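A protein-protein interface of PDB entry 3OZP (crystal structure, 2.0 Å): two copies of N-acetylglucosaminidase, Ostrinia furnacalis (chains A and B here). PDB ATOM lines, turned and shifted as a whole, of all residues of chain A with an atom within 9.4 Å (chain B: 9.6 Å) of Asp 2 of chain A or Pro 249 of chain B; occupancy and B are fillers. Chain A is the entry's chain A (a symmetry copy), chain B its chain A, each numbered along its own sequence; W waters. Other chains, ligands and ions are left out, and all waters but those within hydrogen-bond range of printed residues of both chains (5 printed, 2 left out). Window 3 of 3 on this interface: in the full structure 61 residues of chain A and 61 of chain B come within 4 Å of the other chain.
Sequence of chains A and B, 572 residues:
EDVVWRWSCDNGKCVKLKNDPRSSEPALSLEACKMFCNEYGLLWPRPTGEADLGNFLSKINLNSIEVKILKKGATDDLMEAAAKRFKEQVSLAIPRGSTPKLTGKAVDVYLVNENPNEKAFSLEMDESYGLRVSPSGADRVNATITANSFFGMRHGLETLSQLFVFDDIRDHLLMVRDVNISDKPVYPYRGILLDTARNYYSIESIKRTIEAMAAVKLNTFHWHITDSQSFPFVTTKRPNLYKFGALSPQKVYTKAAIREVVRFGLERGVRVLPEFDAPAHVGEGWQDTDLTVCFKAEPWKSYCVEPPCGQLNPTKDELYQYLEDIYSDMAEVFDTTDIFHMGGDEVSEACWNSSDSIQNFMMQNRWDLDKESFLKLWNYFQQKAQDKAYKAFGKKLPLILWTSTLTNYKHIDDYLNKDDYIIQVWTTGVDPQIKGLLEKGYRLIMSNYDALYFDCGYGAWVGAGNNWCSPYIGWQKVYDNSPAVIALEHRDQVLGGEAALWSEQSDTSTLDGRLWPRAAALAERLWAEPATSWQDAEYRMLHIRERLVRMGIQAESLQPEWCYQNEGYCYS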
ATOM      1  N   GLU A   1     -15.362  26.545  20.838  1.00  0.00           N
ATOM      2  CA  GLU A   1     -15.999  26.013  19.597  1.00  0.00           C
ATOM      3  C   GLU A   1     -17.397  25.448  19.850  1.00  0.00           C
ATOM      4  O   GLU A   1     -17.665  24.254  19.659  1.00  0.00           O
ATOM      5  CB  GLU A   1     -15.080  25.004  18.904  1.00  0.00           C
ATOM      6  CG  GLU A   1     -14.187  25.613  17.817  1.00  0.00           C
ATOM      7  CD  GLU A   1     -13.940  27.111  17.997  1.00  0.00           C
ATOM      8  OE1 GLU A   1     -12.887  27.476  18.565  1.00  0.00           O
ATOM      9  OE2 GLU A   1     -14.803  27.922  17.579  1.00  0.00           O
ATOM     10  N   ASP A   2     -18.278  26.338  20.292  1.00  0.00           N
ATOM     11  CA  ASP A   2     -19.678  26.023  20.507  1.00  0.00           C
ATOM     12  C   ASP A   2     -20.499  26.844  19.529  1.00  0.00           C
ATOM     13  O   ASP A   2     -20.051  27.902  19.080  1.00  0.00           O
ATOM     14  CB  ASP A   2     -20.076  26.355  21.945  1.00  0.00           C
ATOM     15  CG  ASP A   2     -19.279  25.561  22.963  1.00  0.00           C
ATOM     16  OD1 ASP A   2     -18.393  26.156  23.618  1.00  0.00           O
ATOM     17  OD2 ASP A   2     -19.524  24.339  23.090  1.00  0.00           O
ATOM     18  N   VAL A   3     -21.686  26.352  19.188  1.00  0.00           N
ATOM     19  CA  VAL A   3     -22.570  27.069  18.269  1.00  0.00           C
ATOM     20  C   VAL A   3     -22.921  28.469  18.790  1.00  0.00           C
ATOM     21  O   VAL A   3     -23.145  28.676  19.990  1.00  0.00           O
ATOM     22  CB  VAL A   3     -23.808  26.217  17.805  1.00  0.00           C
ATOM     23  CG1 VAL A   3     -23.976  24.968  18.640  1.00  0.00           C
ATOM     24  CG2 VAL A   3     -25.097  27.040  17.722  1.00  0.00           C
ATOM     25  N   VAL A   4     -22.927  29.415  17.857  1.00  0.00           N
ATOM     26  CA  VAL A   4     -23.006  30.841  18.136  1.00  0.00           C
ATOM     27  C   VAL A   4     -24.421  31.375  17.901  1.00  0.00           C
ATOM     28  O   VAL A   4     -24.762  32.479  18.330  1.00  0.00           O
ATOM     29  CB  VAL A   4     -21.938  31.583  17.265  1.00  0.00           C
ATOM     30  CG1 VAL A   4     -22.496  32.812  16.546  1.00  0.00           C
ATOM     31  CG2 VAL A   4     -20.708  31.918  18.095  1.00  0.00           C
ATOM     32  N   TRP A   5     -25.238  30.571  17.228  1.00  0.00           N
ATOM     33  CA  TRP A   5     -26.557  30.997  16.782  1.00  0.00           C
ATOM     34  C   TRP A   5     -27.687  30.333  17.561  1.00  0.00           C
ATOM     35  O   TRP A   5     -27.483  29.338  18.251  1.00  0.00           O
ATOM     36  CB  TRP A   5     -26.726  30.698  15.287  1.00  0.00           C
ATOM     37  CG  TRP A   5     -25.700  31.369  14.434  1.00  0.00           C
ATOM     38  CD1 TRP A   5     -24.583  30.801  13.892  1.00  0.00           C
ATOM     39  CD2 TRP A   5     -25.682  32.745  14.041  1.00  0.00           C
ATOM     40  NE1 TRP A   5     -23.872  31.736  13.180  1.00  0.00           N
ATOM     41  CE2 TRP A   5     -24.527  32.939  13.249  1.00  0.00           C
ATOM     42  CE3 TRP A   5     -26.537  33.833  14.271  1.00  0.00           C
ATOM     43  CZ2 TRP A   5     -24.197  34.179  12.693  1.00  0.00           C
ATOM     44  CZ3 TRP A   5     -26.210  35.071  13.712  1.00  0.00           C
ATOM     45  CH2 TRP A   5     -25.047  35.230  12.935  1.00  0.00           C
ATOM     46  N   TRP A   7     -32.265  29.777  16.954  1.00  0.00           N
ATOM     47  CA  TRP A   7     -33.342  29.881  15.986  1.00  0.00           C
ATOM     48  C   TRP A   7     -34.675  30.161  16.671  1.00  0.00           C
ATOM     49  O   TRP A   7     -34.932  29.680  17.776  1.00  0.00           O
ATOM     50  CB  TRP A   7     -33.414  28.616  15.122  1.00  0.00           C
ATOM     51  CG  TRP A   7     -32.308  28.544  14.102  1.00  0.00           C
ATOM     52  CD1 TRP A   7     -32.390  28.879  12.780  1.00  0.00           C
ATOM     53  CD2 TRP A   7     -30.956  28.130  14.327  1.00  0.00           C
ATOM     54  NE1 TRP A   7     -31.174  28.693  12.166  1.00  0.00           N
ATOM     55  CE2 TRP A   7     -30.275  28.234  13.092  1.00  0.00           C
ATOM     56  CE3 TRP A   7     -30.252  27.671  15.451  1.00  0.00           C
ATOM     57  CZ2 TRP A   7     -28.924  27.902  12.947  1.00  0.00           C
ATOM     58  CZ3 TRP A   7     -28.904  27.338  15.307  1.00  0.00           C
ATOM     59  CH2 TRP A   7     -28.258  27.453  14.060  1.00  0.00           C
ATOM     60  N   ASN A  19     -27.247  34.339  19.280  1.00  0.00           N
ATOM     61  CA  ASN A  19     -27.528  33.923  20.649  1.00  0.00           C
ATOM     62  C   ASN A  19     -26.834  34.891  21.606  1.00  0.00           C
ATOM     63  O   ASN A  19     -25.767  34.596  22.144  1.00  0.00           O
ATOM     64  CB  ASN A  19     -27.087  32.471  20.884  1.00  0.00           C
ATOM     65  CG  ASN A  19     -27.506  31.931  22.254  1.00  0.00           C
ATOM     66  OD1 ASN A  19     -26.917  30.971  22.755  1.00  0.00           O
ATOM     67  ND2 ASN A  19     -28.527  32.537  22.855  1.00  0.00           N
ATOM     68  N   SER A  98     -20.286  14.313  18.134  1.00  0.00           N
ATOM     69  CA  SER A  98     -20.971  14.883  19.292  1.00  0.00           C
ATOM     70  C   SER A  98     -21.391  13.790  20.268  1.00  0.00           C
ATOM     71  O   SER A  98     -21.766  12.691  19.856  1.00  0.00           O
ATOM     72  CB  SER A  98     -22.197  15.689  18.855  1.00  0.00           C
ATOM     73  OG  SER A  98     -21.822  16.860  18.155  1.00  0.00           O
ATOM     74  N   LYS A 101     -25.006  14.601  26.965  1.00  0.00           N
ATOM     75  CA  LYS A 101     -24.835  14.456  28.404  1.00  0.00           C
ATOM     76  C   LYS A 101     -25.775  13.366  28.902  1.00  0.00           C
ATOM     77  O   LYS A 101     -26.964  13.359  28.566  1.00  0.00           O
ATOM     78  CB  LYS A 101     -25.093  15.781  29.125  1.00  0.00           C
ATOM     79  CG  LYS A 101     -24.035  16.841  28.853  1.00  0.00           C
ATOM     80  CD  LYS A 101     -24.176  18.022  29.794  1.00  0.00           C
ATOM     81  CE  LYS A 101     -23.073  19.048  29.575  1.00  0.00           C
ATOM     82  NZ  LYS A 101     -23.237  19.828  28.307  1.00  0.00           N
ATOM     83  N   ASP A 167     -29.926  18.693  20.899  1.00  0.00           N
ATOM     84  CA  ASP A 167     -29.660  20.105  21.147  1.00  0.00           C
ATOM     85  C   ASP A 167     -28.151  20.272  21.152  1.00  0.00           C
ATOM     86  O   ASP A 167     -27.487  19.886  22.112  1.00  0.00           O
ATOM     87  CB  ASP A 167     -30.258  20.517  22.503  1.00  0.00           C
ATOM     88  CG  ASP A 167     -30.079  22.003  22.816  1.00  0.00           C
ATOM     89  OD1 ASP A 167     -30.970  22.569  23.483  1.00  0.00           O
ATOM     90  OD2 ASP A 167     -29.063  22.607  22.415  1.00  0.00           O
ATOM     91  N   ASP A 168     -27.608  20.837  20.076  1.00  0.00           N
ATOM     92  CA  ASP A 168     -26.155  20.982  19.947  1.00  0.00           C
ATOM     93  C   ASP A 168     -25.621  22.264  20.590  1.00  0.00           C
ATOM     94  O   ASP A 168     -24.410  22.482  20.635  1.00  0.00           O
ATOM     95  CB  ASP A 168     -25.701  20.854  18.483  1.00  0.00           C
ATOM     96  CG  ASP A 168     -26.375  21.858  17.556  1.00  0.00           C
ATOM     97  OD1 ASP A 168     -25.910  21.976  16.405  1.00  0.00           O
ATOM     98  OD2 ASP A 168     -27.358  22.524  17.950  1.00  0.00           O
ATOM     99  N   ILE A 169     -26.528  23.099  21.088  1.00  0.00           N
ATOM    100  CA  ILE A 169     -26.148  24.259  21.895  1.00  0.00           C
ATOM    101  C   ILE A 169     -25.763  23.783  23.302  1.00  0.00           C
ATOM    102  O   ILE A 169     -24.737  24.195  23.844  1.00  0.00           O
ATOM    103  CB  ILE A 169     -27.278  25.329  21.937  1.00  0.00           C
ATOM    104  CG1 ILE A 169     -27.511  25.914  20.537  1.00  0.00           C
ATOM    105  CG2 ILE A 169     -26.943  26.443  22.928  1.00  0.00           C
ATOM    106  CD1 ILE A 169     -28.693  26.871  20.429  1.00  0.00           C
ATOM    107  N   ARG A 170     -26.573  22.882  23.857  1.00  0.00           N
ATOM    108  CA  ARG A 170     -26.400  22.389  25.225  1.00  0.00           C
ATOM    109  C   ARG A 170     -25.825  20.968  25.322  1.00  0.00           C
ATOM    110  O   ARG A 170     -25.497  20.508  26.419  1.00  0.00           O
ATOM    111  CB  ARG A 170     -27.739  22.447  25.969  1.00  0.00           C
ATOM    112  CG  ARG A 170     -28.293  23.847  26.163  1.00  0.00           C
ATOM    113  CD  ARG A 170     -29.704  23.814  26.743  1.00  0.00           C
ATOM    114  NE  ARG A 170     -30.316  25.142  26.770  1.00  0.00           N
ATOM    115  CZ  ARG A 170     -30.868  25.745  25.719  1.00  0.00           C
ATOM    116  NH1 ARG A 170     -31.394  26.957  25.857  1.00  0.00           N
ATOM    117  NH2 ARG A 170     -30.890  25.151  24.525  1.00  0.00           N
ATOM    118  N   ASP A 171     -25.693  20.289  24.179  1.00  0.00           N
ATOM    119  CA  ASP A 171     -25.340  18.858  24.125  1.00  0.00           C
ATOM    120  C   ASP A 171     -26.349  17.977  24.885  1.00  0.00           C
ATOM    121  O   ASP A 171     -25.961  17.082  25.638  1.00  0.00           O
ATOM    122  CB  ASP A 171     -23.906  18.599  24.617  1.00  0.00           C
ATOM    123  CG  ASP A 171     -22.846  19.073  23.638  1.00  0.00           C
ATOM    124  OD1 ASP A 171     -23.046  18.952  22.408  1.00  0.00           O
ATOM    125  OD2 ASP A 171     -21.795  19.559  24.108  1.00  0.00           O
ATOM    126  N   GLU A 561     -26.621  23.921   2.640  1.00  0.00           N
ATOM    127  CA  GLU A 561     -27.008  23.766   4.042  1.00  0.00           C
ATOM    128  C   GLU A 561     -27.490  25.096   4.624  1.00  0.00           C
ATOM    129  O   GLU A 561     -28.342  25.117   5.517  1.00  0.00           O
ATOM    130  CB  GLU A 561     -25.867  23.180   4.877  1.00  0.00           C
ATOM    131  CG  GLU A 561     -26.308  22.745   6.280  1.00  0.00           C
ATOM    132  CD  GLU A 561     -25.266  21.929   7.026  1.00  0.00           C
ATOM    133  OE1 GLU A 561     -24.189  21.628   6.465  1.00  0.00           O
ATOM    134  OE2 GLU A 561     -25.532  21.575   8.191  1.00  0.00           O
ATOM    135  N   GLN A 565     -30.610  26.009   7.248  1.00  0.00           N
ATOM    136  CA  GLN A 565     -30.447  26.841   8.439  1.00  0.00           C
ATOM    137  C   GLN A 565     -31.214  28.163   8.376  1.00  0.00           C
ATOM    138  O   GLN A 565     -31.373  28.835   9.396  1.00  0.00           O
ATOM    139  CB  GLN A 565     -28.962  27.111   8.702  1.00  0.00           C
ATOM    140  CG  GLN A 565     -28.192  25.868   9.119  1.00  0.00           C
ATOM    141  CD  GLN A 565     -26.798  26.154   9.618  1.00  0.00           C
ATOM    142  OE1 GLN A 565     -26.035  25.226   9.891  1.00  0.00           O
ATOM    143  NE2 GLN A 565     -26.449  27.430   9.746  1.00  0.00           N
ATOM    144  N   TYR B 200     -20.277  22.016   3.075  1.00  0.00           N
ATOM    145  CA  TYR B 200     -18.995  21.614   3.648  1.00  0.00           C
ATOM    146  C   TYR B 200     -18.508  20.272   3.100  1.00  0.00           C
ATOM    147  O   TYR B 200     -19.303  19.384   2.808  1.00  0.00           O
ATOM    148  CB  TYR B 200     -19.094  21.577   5.174  1.00  0.00           C
ATOM    149  CG  TYR B 200     -17.792  21.323   5.886  1.00  0.00           C
ATOM    150  CD1 TYR B 200     -17.494  20.059   6.390  1.00  0.00           C
ATOM    151  CD2 TYR B 200     -16.857  22.342   6.060  1.00  0.00           C
ATOM    152  CE1 TYR B 200     -16.306  19.813   7.049  1.00  0.00           C
ATOM    153  CE2 TYR B 200     -15.656  22.102   6.727  1.00  0.00           C
ATOM    154  CZ  TYR B 200     -15.395  20.835   7.218  1.00  0.00           C
ATOM    155  OH  TYR B 200     -14.219  20.580   7.875  1.00  0.00           O
ATOM    156  N   PHE B 231     -18.388  30.808   5.822  1.00  0.00           N
ATOM    157  CA  PHE B 231     -16.983  31.151   5.935  1.00  0.00           C
ATOM    158  C   PHE B 231     -16.318  30.077   6.809  1.00  0.00           C
ATOM    159  O   PHE B 231     -16.207  30.253   8.024  1.00  0.00           O
ATOM    160  CB  PHE B 231     -16.855  32.541   6.583  1.00  0.00           C
ATOM    161  CG  PHE B 231     -15.516  33.206   6.377  1.00  0.00           C
ATOM    162  CD1 PHE B 231     -15.423  34.381   5.642  1.00  0.00           C
ATOM    163  CD2 PHE B 231     -14.356  32.676   6.934  1.00  0.00           C
ATOM    164  CE1 PHE B 231     -14.198  35.013   5.456  1.00  0.00           C
ATOM    165  CE2 PHE B 231     -13.124  33.297   6.745  1.00  0.00           C
ATOM    166  CZ  PHE B 231     -13.045  34.468   6.010  1.00  0.00           C
ATOM    167  N   PRO B 232     -15.903  28.943   6.202  1.00  0.00           N
ATOM    168  CA  PRO B 232     -15.280  27.865   6.980  1.00  0.00           C
ATOM    169  C   PRO B 232     -13.780  28.037   7.201  1.00  0.00           C
ATOM    170  O   PRO B 232     -13.194  27.312   8.011  1.00  0.00           O
ATOM    171  CB  PRO B 232     -15.550  26.621   6.125  1.00  0.00           C
ATOM    172  CG  PRO B 232     -15.561  27.140   4.718  1.00  0.00           C
ATOM    173  CD  PRO B 232     -16.148  28.539   4.802  1.00  0.00           C
ATOM    174  N   VAL B 234     -10.570  29.189   8.774  1.00  0.00           N
ATOM    175  CA  VAL B 234     -10.178  29.688  10.091  1.00  0.00           C
ATOM    176  C   VAL B 234      -9.130  30.801   9.962  1.00  0.00           C
ATOM    177  O   VAL B 234      -7.938  30.530   9.764  1.00  0.00           O
ATOM    178  CB  VAL B 234      -9.706  28.550  11.039  1.00  0.00           C
ATOM    179  CG1 VAL B 234      -9.130  29.118  12.342  1.00  0.00           C
ATOM    180  CG2 VAL B 234     -10.863  27.615  11.348  1.00  0.00           C
ATOM    181  N   TYR B 242     -15.130  33.288  10.854  1.00  0.00           N
ATOM    182  CA  TYR B 242     -15.455  31.862  10.858  1.00  0.00           C
ATOM    183  C   TYR B 242     -16.366  31.455  12.021  1.00  0.00           C
ATOM    184  O   TYR B 242     -17.178  30.544  11.874  1.00  0.00           O
ATOM    185  CB  TYR B 242     -14.200  30.984  10.781  1.00  0.00           C
ATOM    186  CG  TYR B 242     -13.397  30.854  12.058  1.00  0.00           C
ATOM    187  CD1 TYR B 242     -13.723  29.889  13.014  1.00  0.00           C
ATOM    188  CD2 TYR B 242     -12.288  31.668  12.294  1.00  0.00           C
ATOM    189  CE1 TYR B 242     -12.985  29.755  14.181  1.00  0.00           C
ATOM    190  CE2 TYR B 242     -11.541  31.541  13.458  1.00  0.00           C
ATOM    191  CZ  TYR B 242     -11.901  30.586  14.399  1.00  0.00           C
ATOM    192  OH  TYR B 242     -11.166  30.451  15.550  1.00  0.00           O
ATOM    193  N   LYS B 243     -16.245  32.137  13.160  1.00  0.00           N
ATOM    194  CA  LYS B 243     -17.153  31.884  14.285  1.00  0.00           C
ATOM    195  C   LYS B 243     -18.608  32.162  13.912  1.00  0.00           C
ATOM    196  O   LYS B 243     -19.478  31.346  14.197  1.00  0.00           O
ATOM    197  CB  LYS B 243     -16.748  32.673  15.534  1.00  0.00           C
ATOM    198  CG  LYS B 243     -15.503  32.125  16.226  1.00  0.00           C
ATOM    199  CD  LYS B 243     -15.264  32.804  17.570  1.00  0.00           C
ATOM    200  CE  LYS B 243     -13.780  32.855  17.913  1.00  0.00           C
ATOM    201  NZ  LYS B 243     -13.121  31.514  17.865  1.00  0.00           N
ATOM    202  N   PHE B 244     -18.866  33.299  13.266  1.00  0.00           N
ATOM    203  CA  PHE B 244     -20.222  33.624  12.819  1.00  0.00           C
ATOM    204  C   PHE B 244     -20.554  32.958  11.485  1.00  0.00           C
ATOM    205  O   PHE B 244     -21.721  32.690  11.200  1.00  0.00           O
ATOM    206  CB  PHE B 244     -20.442  35.136  12.668  1.00  0.00           C
ATOM    207  CG  PHE B 244     -20.172  35.946  13.916  1.00  0.00           C
ATOM    208  CD1 PHE B 244     -20.119  35.353  15.177  1.00  0.00           C
ATOM    209  CD2 PHE B 244     -20.001  37.327  13.819  1.00  0.00           C
ATOM    210  CE1 PHE B 244     -19.871  36.118  16.321  1.00  0.00           C
ATOM    211  CE2 PHE B 244     -19.762  38.104  14.957  1.00  0.00           C
ATOM    212  CZ  PHE B 244     -19.697  37.494  16.209  1.00  0.00           C
ATOM    213  N   GLY B 245     -19.525  32.708  10.675  1.00  0.00           N
ATOM    214  CA  GLY B 245     -19.708  32.295   9.288  1.00  0.00           C
ATOM    215  C   GLY B 245     -19.829  30.810   9.017  1.00  0.00           C
ATOM    216  O   GLY B 245     -20.436  30.418   8.027  1.00  0.00           O
ATOM    217  N   ALA B 246     -19.251  29.982   9.881  1.00  0.00           N
ATOM    218  CA  ALA B 246     -19.263  28.531   9.667  1.00  0.00           C
ATOM    219  C   ALA B 246     -20.666  27.949   9.831  1.00  0.00           C
ATOM    220  O   ALA B 246     -21.486  28.491  10.578  1.00  0.00           O
ATOM    221  CB  ALA B 246     -18.280  27.846  10.598  1.00  0.00           C
ATOM    222  N   LEU B 247     -20.947  26.868   9.106  1.00  0.00           N
ATOM    223  CA  LEU B 247     -22.242  26.187   9.192  1.00  0.00           C
ATOM    224  C   LEU B 247     -22.407  25.516  10.554  1.00  0.00           C
ATOM    225  O   LEU B 247     -23.525  25.318  11.028  1.00  0.00           O
ATOM    226  CB  LEU B 247     -22.402  25.162   8.057  1.00  0.00           C
ATOM    227  CG  LEU B 247     -22.525  25.706   6.625  1.00  0.00           C
ATOM    228  CD1 LEU B 247     -22.253  24.602   5.592  1.00  0.00           C
ATOM    229  CD2 LEU B 247     -23.893  26.344   6.388  1.00  0.00           C
ATOM    230  N   SER B 248     -21.277  25.177  11.167  1.00  0.00           N
ATOM    231  CA  SER B 248     -21.216  24.630  12.517  1.00  0.00           C
ATOM    232  C   SER B 248     -19.767  24.761  12.976  1.00  0.00           C
ATOM    233  O   SER B 248     -18.882  24.969  12.141  1.00  0.00           O
ATOM    234  CB  SER B 248     -21.658  23.160  12.528  1.00  0.00           C
ATOM    235  OG  SER B 248     -20.570  22.289  12.258  1.00  0.00           O
ATOM    236  N   PRO B 249     -19.511  24.647  14.299  1.00  0.00           N
ATOM    237  CA  PRO B 249     -18.150  24.758  14.825  1.00  0.00           C
ATOM    238  C   PRO B 249     -17.207  23.683  14.299  1.00  0.00           C
ATOM    239  O   PRO B 249     -16.000  23.905  14.253  1.00  0.00           O
ATOM    240  CB  PRO B 249     -18.345  24.585  16.340  1.00  0.00           C
ATOM    241  CG  PRO B 249     -19.749  24.992  16.585  1.00  0.00           C
ATOM    242  CD  PRO B 249     -20.498  24.500  15.388  1.00  0.00           C
ATOM    243  N   GLN B 250     -17.750  22.530  13.923  1.00  0.00           N
ATOM    244  CA  GLN B 250     -16.951  21.427  13.396  1.00  0.00           C
ATOM    245  C   GLN B 250     -16.750  21.539  11.883  1.00  0.00           C
ATOM    246  O   GLN B 250     -15.809  20.957  11.337  1.00  0.00           O
ATOM    247  CB  GLN B 250     -17.583  20.074  13.745  1.00  0.00           C
ATOM    248  CG  GLN B 250     -17.706  19.791  15.254  1.00  0.00           C
ATOM    249  CD  GLN B 250     -18.878  20.516  15.913  1.00  0.00           C
ATOM    250  OE1 GLN B 250     -19.844  20.904  15.248  1.00  0.00           O
ATOM    251  NE2 GLN B 250     -18.797  20.697  17.232  1.00  0.00           N
ATOM    252  N   LYS B 251     -17.630  22.290  11.219  1.00  0.00           N
ATOM    253  CA  LYS B 251     -17.563  22.476   9.770  1.00  0.00           C
ATOM    254  C   LYS B 251     -16.669  23.665   9.437  1.00  0.00           C
ATOM    255  O   LYS B 251     -17.111  24.723   8.994  1.00  0.00           O
ATOM    256  CB  LYS B 251     -18.965  22.588   9.167  1.00  0.00           C
ATOM    257  CG  LYS B 251     -19.675  21.245   9.176  1.00  0.00           C
ATOM    258  CD  LYS B 251     -21.045  21.287   8.539  1.00  0.00           C
ATOM    259  CE  LYS B 251     -21.608  19.875   8.480  1.00  0.00           C
ATOM    260  NZ  LYS B 251     -23.061  19.857   8.202  1.00  0.00           N
ATOM    261  N   VAL B 252     -15.380  23.437   9.649  1.00  0.00           N
ATOM    262  CA  VAL B 252     -14.384  24.472   9.643  1.00  0.00           C
ATOM    263  C   VAL B 252     -13.098  23.886   9.053  1.00  0.00           C
ATOM    264  O   VAL B 252     -12.913  22.665   9.049  1.00  0.00           O
ATOM    265  CB  VAL B 252     -14.223  24.984  11.104  1.00  0.00           C
ATOM    266  CG1 VAL B 252     -12.811  24.827  11.651  1.00  0.00           C
ATOM    267  CG2 VAL B 252     -14.810  26.389  11.260  1.00  0.00           C
ATOM    268  N   TYR B 253     -12.238  24.754   8.526  1.00  0.00           N
ATOM    269  CA  TYR B 253     -10.920  24.352   8.052  1.00  0.00           C
ATOM    270  C   TYR B 253      -9.840  25.078   8.843  1.00  0.00           C
ATOM    271  O   TYR B 253      -9.516  26.237   8.563  1.00  0.00           O
ATOM    272  CB  TYR B 253     -10.776  24.609   6.543  1.00  0.00           C
ATOM    273  CG  TYR B 253     -11.796  23.875   5.703  1.00  0.00           C
ATOM    274  CD1 TYR B 253     -11.775  22.484   5.611  1.00  0.00           C
ATOM    275  CD2 TYR B 253     -12.775  24.572   4.993  1.00  0.00           C
ATOM    276  CE1 TYR B 253     -12.706  21.800   4.843  1.00  0.00           C
ATOM    277  CE2 TYR B 253     -13.718  23.894   4.211  1.00  0.00           C
ATOM    278  CZ  TYR B 253     -13.672  22.508   4.145  1.00  0.00           C
ATOM    279  OH  TYR B 253     -14.587  21.825   3.384  1.00  0.00           O
ATOM    280  N   THR B 254      -9.304  24.382   9.845  1.00  0.00           N
ATOM    281  CA  THR B 254      -8.282  24.923  10.734  1.00  0.00           C
ATOM    282  C   THR B 254      -6.959  25.057   9.997  1.00  0.00           C
ATOM    283  O   THR B 254      -6.791  24.498   8.911  1.00  0.00           O
ATOM    284  CB  THR B 254      -8.032  23.999  11.945  1.00  0.00           C
ATOM    285  OG1 THR B 254      -7.592  22.717  11.481  1.00  0.00           O
ATOM    286  CG2 THR B 254      -9.287  23.840  12.806  1.00  0.00           C
HETATM  287  O   HOH W   1     -19.782  22.734  19.547  1.00  0.00           O
HETATM  288  O   HOH W   2     -22.836  21.378   4.217  1.00  0.00           O
HETATM  289  O   HOH W   3     -24.095  21.795  10.428  1.00  0.00           O
HETATM  290  O   HOH W   4     -24.657  28.482  11.501  1.00  0.00           O
HETATM  291  O   HOH W   5     -15.223  27.046  15.045  1.00  0.00           O
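Of the printed residues of chain B, Glu 1 of chain A touches Lys 243 (3.98 Å) and Pro 249 (3.4 Å). Asp 2 of chain A touches just one residue of chain B: Pro 249 (3.6 Å). Of the printed residues of chain B, Trp 5 of chain A touches Phe 244. Printed residues of chain B within 4 Å of Glu 561 of chain A: Leu 247 and Lys 251. Phe 231 of chain B touches none of the printed residues of chain A. Ser 248 of chain B touches none of the printed residues of chain A. Of chain A, only Glu 1, Asp 2 and Val 3 come within 4 Å of Pro 249 of chain B. No residue of chain A comes within 4 Å of Gln 250 of chain B. Thr 254 of chain B touches none of the printed residues of chain A.
The side-chain amide oxygen (OE1) of Gln 565 of chain A sits close to the backbone carbonyl oxygen (O) of Leu 247 of chain B (2.8 Å). The side-chain amino group (NZ) of Lys 243 of chain B lies within salt-bridge range of the side-chain carboxylate (OE2) of Glu 1 of chain A. OE1 of Glu 561 of chain A lies within salt-bridge range of NZ of Lys 251 of chain B, 2.7 Å away. NE1 of Trp 5 of chain A sits at hydrogen-bond distance from O of Phe 244 of chain B.
NE1 of Trp 7 of chain A sits at hydrogen-bond distance from O of Gln 565 of chain A, at 2.8 Å. The side-chain hydroxyl (OG) of Ser 248 of chain B is in hydrogen-bond range of the backbone NH (N) of Lys 251 of chain B. NZ of Lys 243 of chain B is in hydrogen-bond range of OH of Tyr 242 of chain B, 3.2 Å away. The backbone carbonyl oxygen (O) of Val 4 of chain A sits at hydrogen-bond distance from the backbone NH (N) of Asn 19 of chain A, at 3.2 Å.
Water W1 bridges the backbone carbonyl oxygen (O) of Glu 1 of chain A (2.6 Å) and the side-chain amide nitrogen (NE2) of Gln 250 of chain B (3.2 Å). Water W2 lies within hydrogen-bond range of OE1 of Glu 561 of chain A (2.6 Å) and N of Tyr 200 of chain B (2.9 Å). Water W3 bridges OE2 of Glu 561 of chain A and NZ of Lys 251 of chain B. Water W5 bridges the side-chain carboxylate (OE2) of Glu 1 of chain A (2.7 Å) and the backbone carbonyl oxygen (O) of Pro 249 of chain B (3.3 Å). Water W4 lies within hydrogen-bond range of the side-chain amide nitrogen (NE2) of Gln 565 of chain A (2.7 Å), the backbone carbonyl oxygen (O) of Ala 246 of chain B (3.3 Å) and the backbone carbonyl oxygen (O) of Leu 247 of chain B (3.4 Å).
Along chain A the printed residues that touch a printed residue of chain B span positions 1 to 565. Of the 17 printed residues of chain B, 5 touch a printed residue of chain A. Printed residues of chain B that touch a printed residue of chain A: Lys 243, Phe 244, Leu 247, Pro 249 and Lys 251. Hydrophobic or aromatic side chains of chain B that line the printed part of chain A: Phe 244, Leu 247 and Pro 249.
No position is printed for both chains. Of the 10 pairs that touch across the chains among the printed residues, none has its exchanged pair printed and touching as well.
Glu 1 of chain A touches Pro 249 of chain B (O to CB, 3.4 Å). Pro 249 of chain B touches Asp 2 of chain A (CG to C, 3.6 Å). Pro 249 of chain B touches Val 3 of chain A (CG to N, 3.5 Å). Lys 243 of chain B touches Val 4 of chain A (O to CB, 3.9 Å). Val 4 of chain A touches Phe 244 of chain B (CG1 to CD1, 3.7 Å). Glu 561 of chain A touches Leu 247 of chain B (OE1 to CD1, 3.7 Å).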
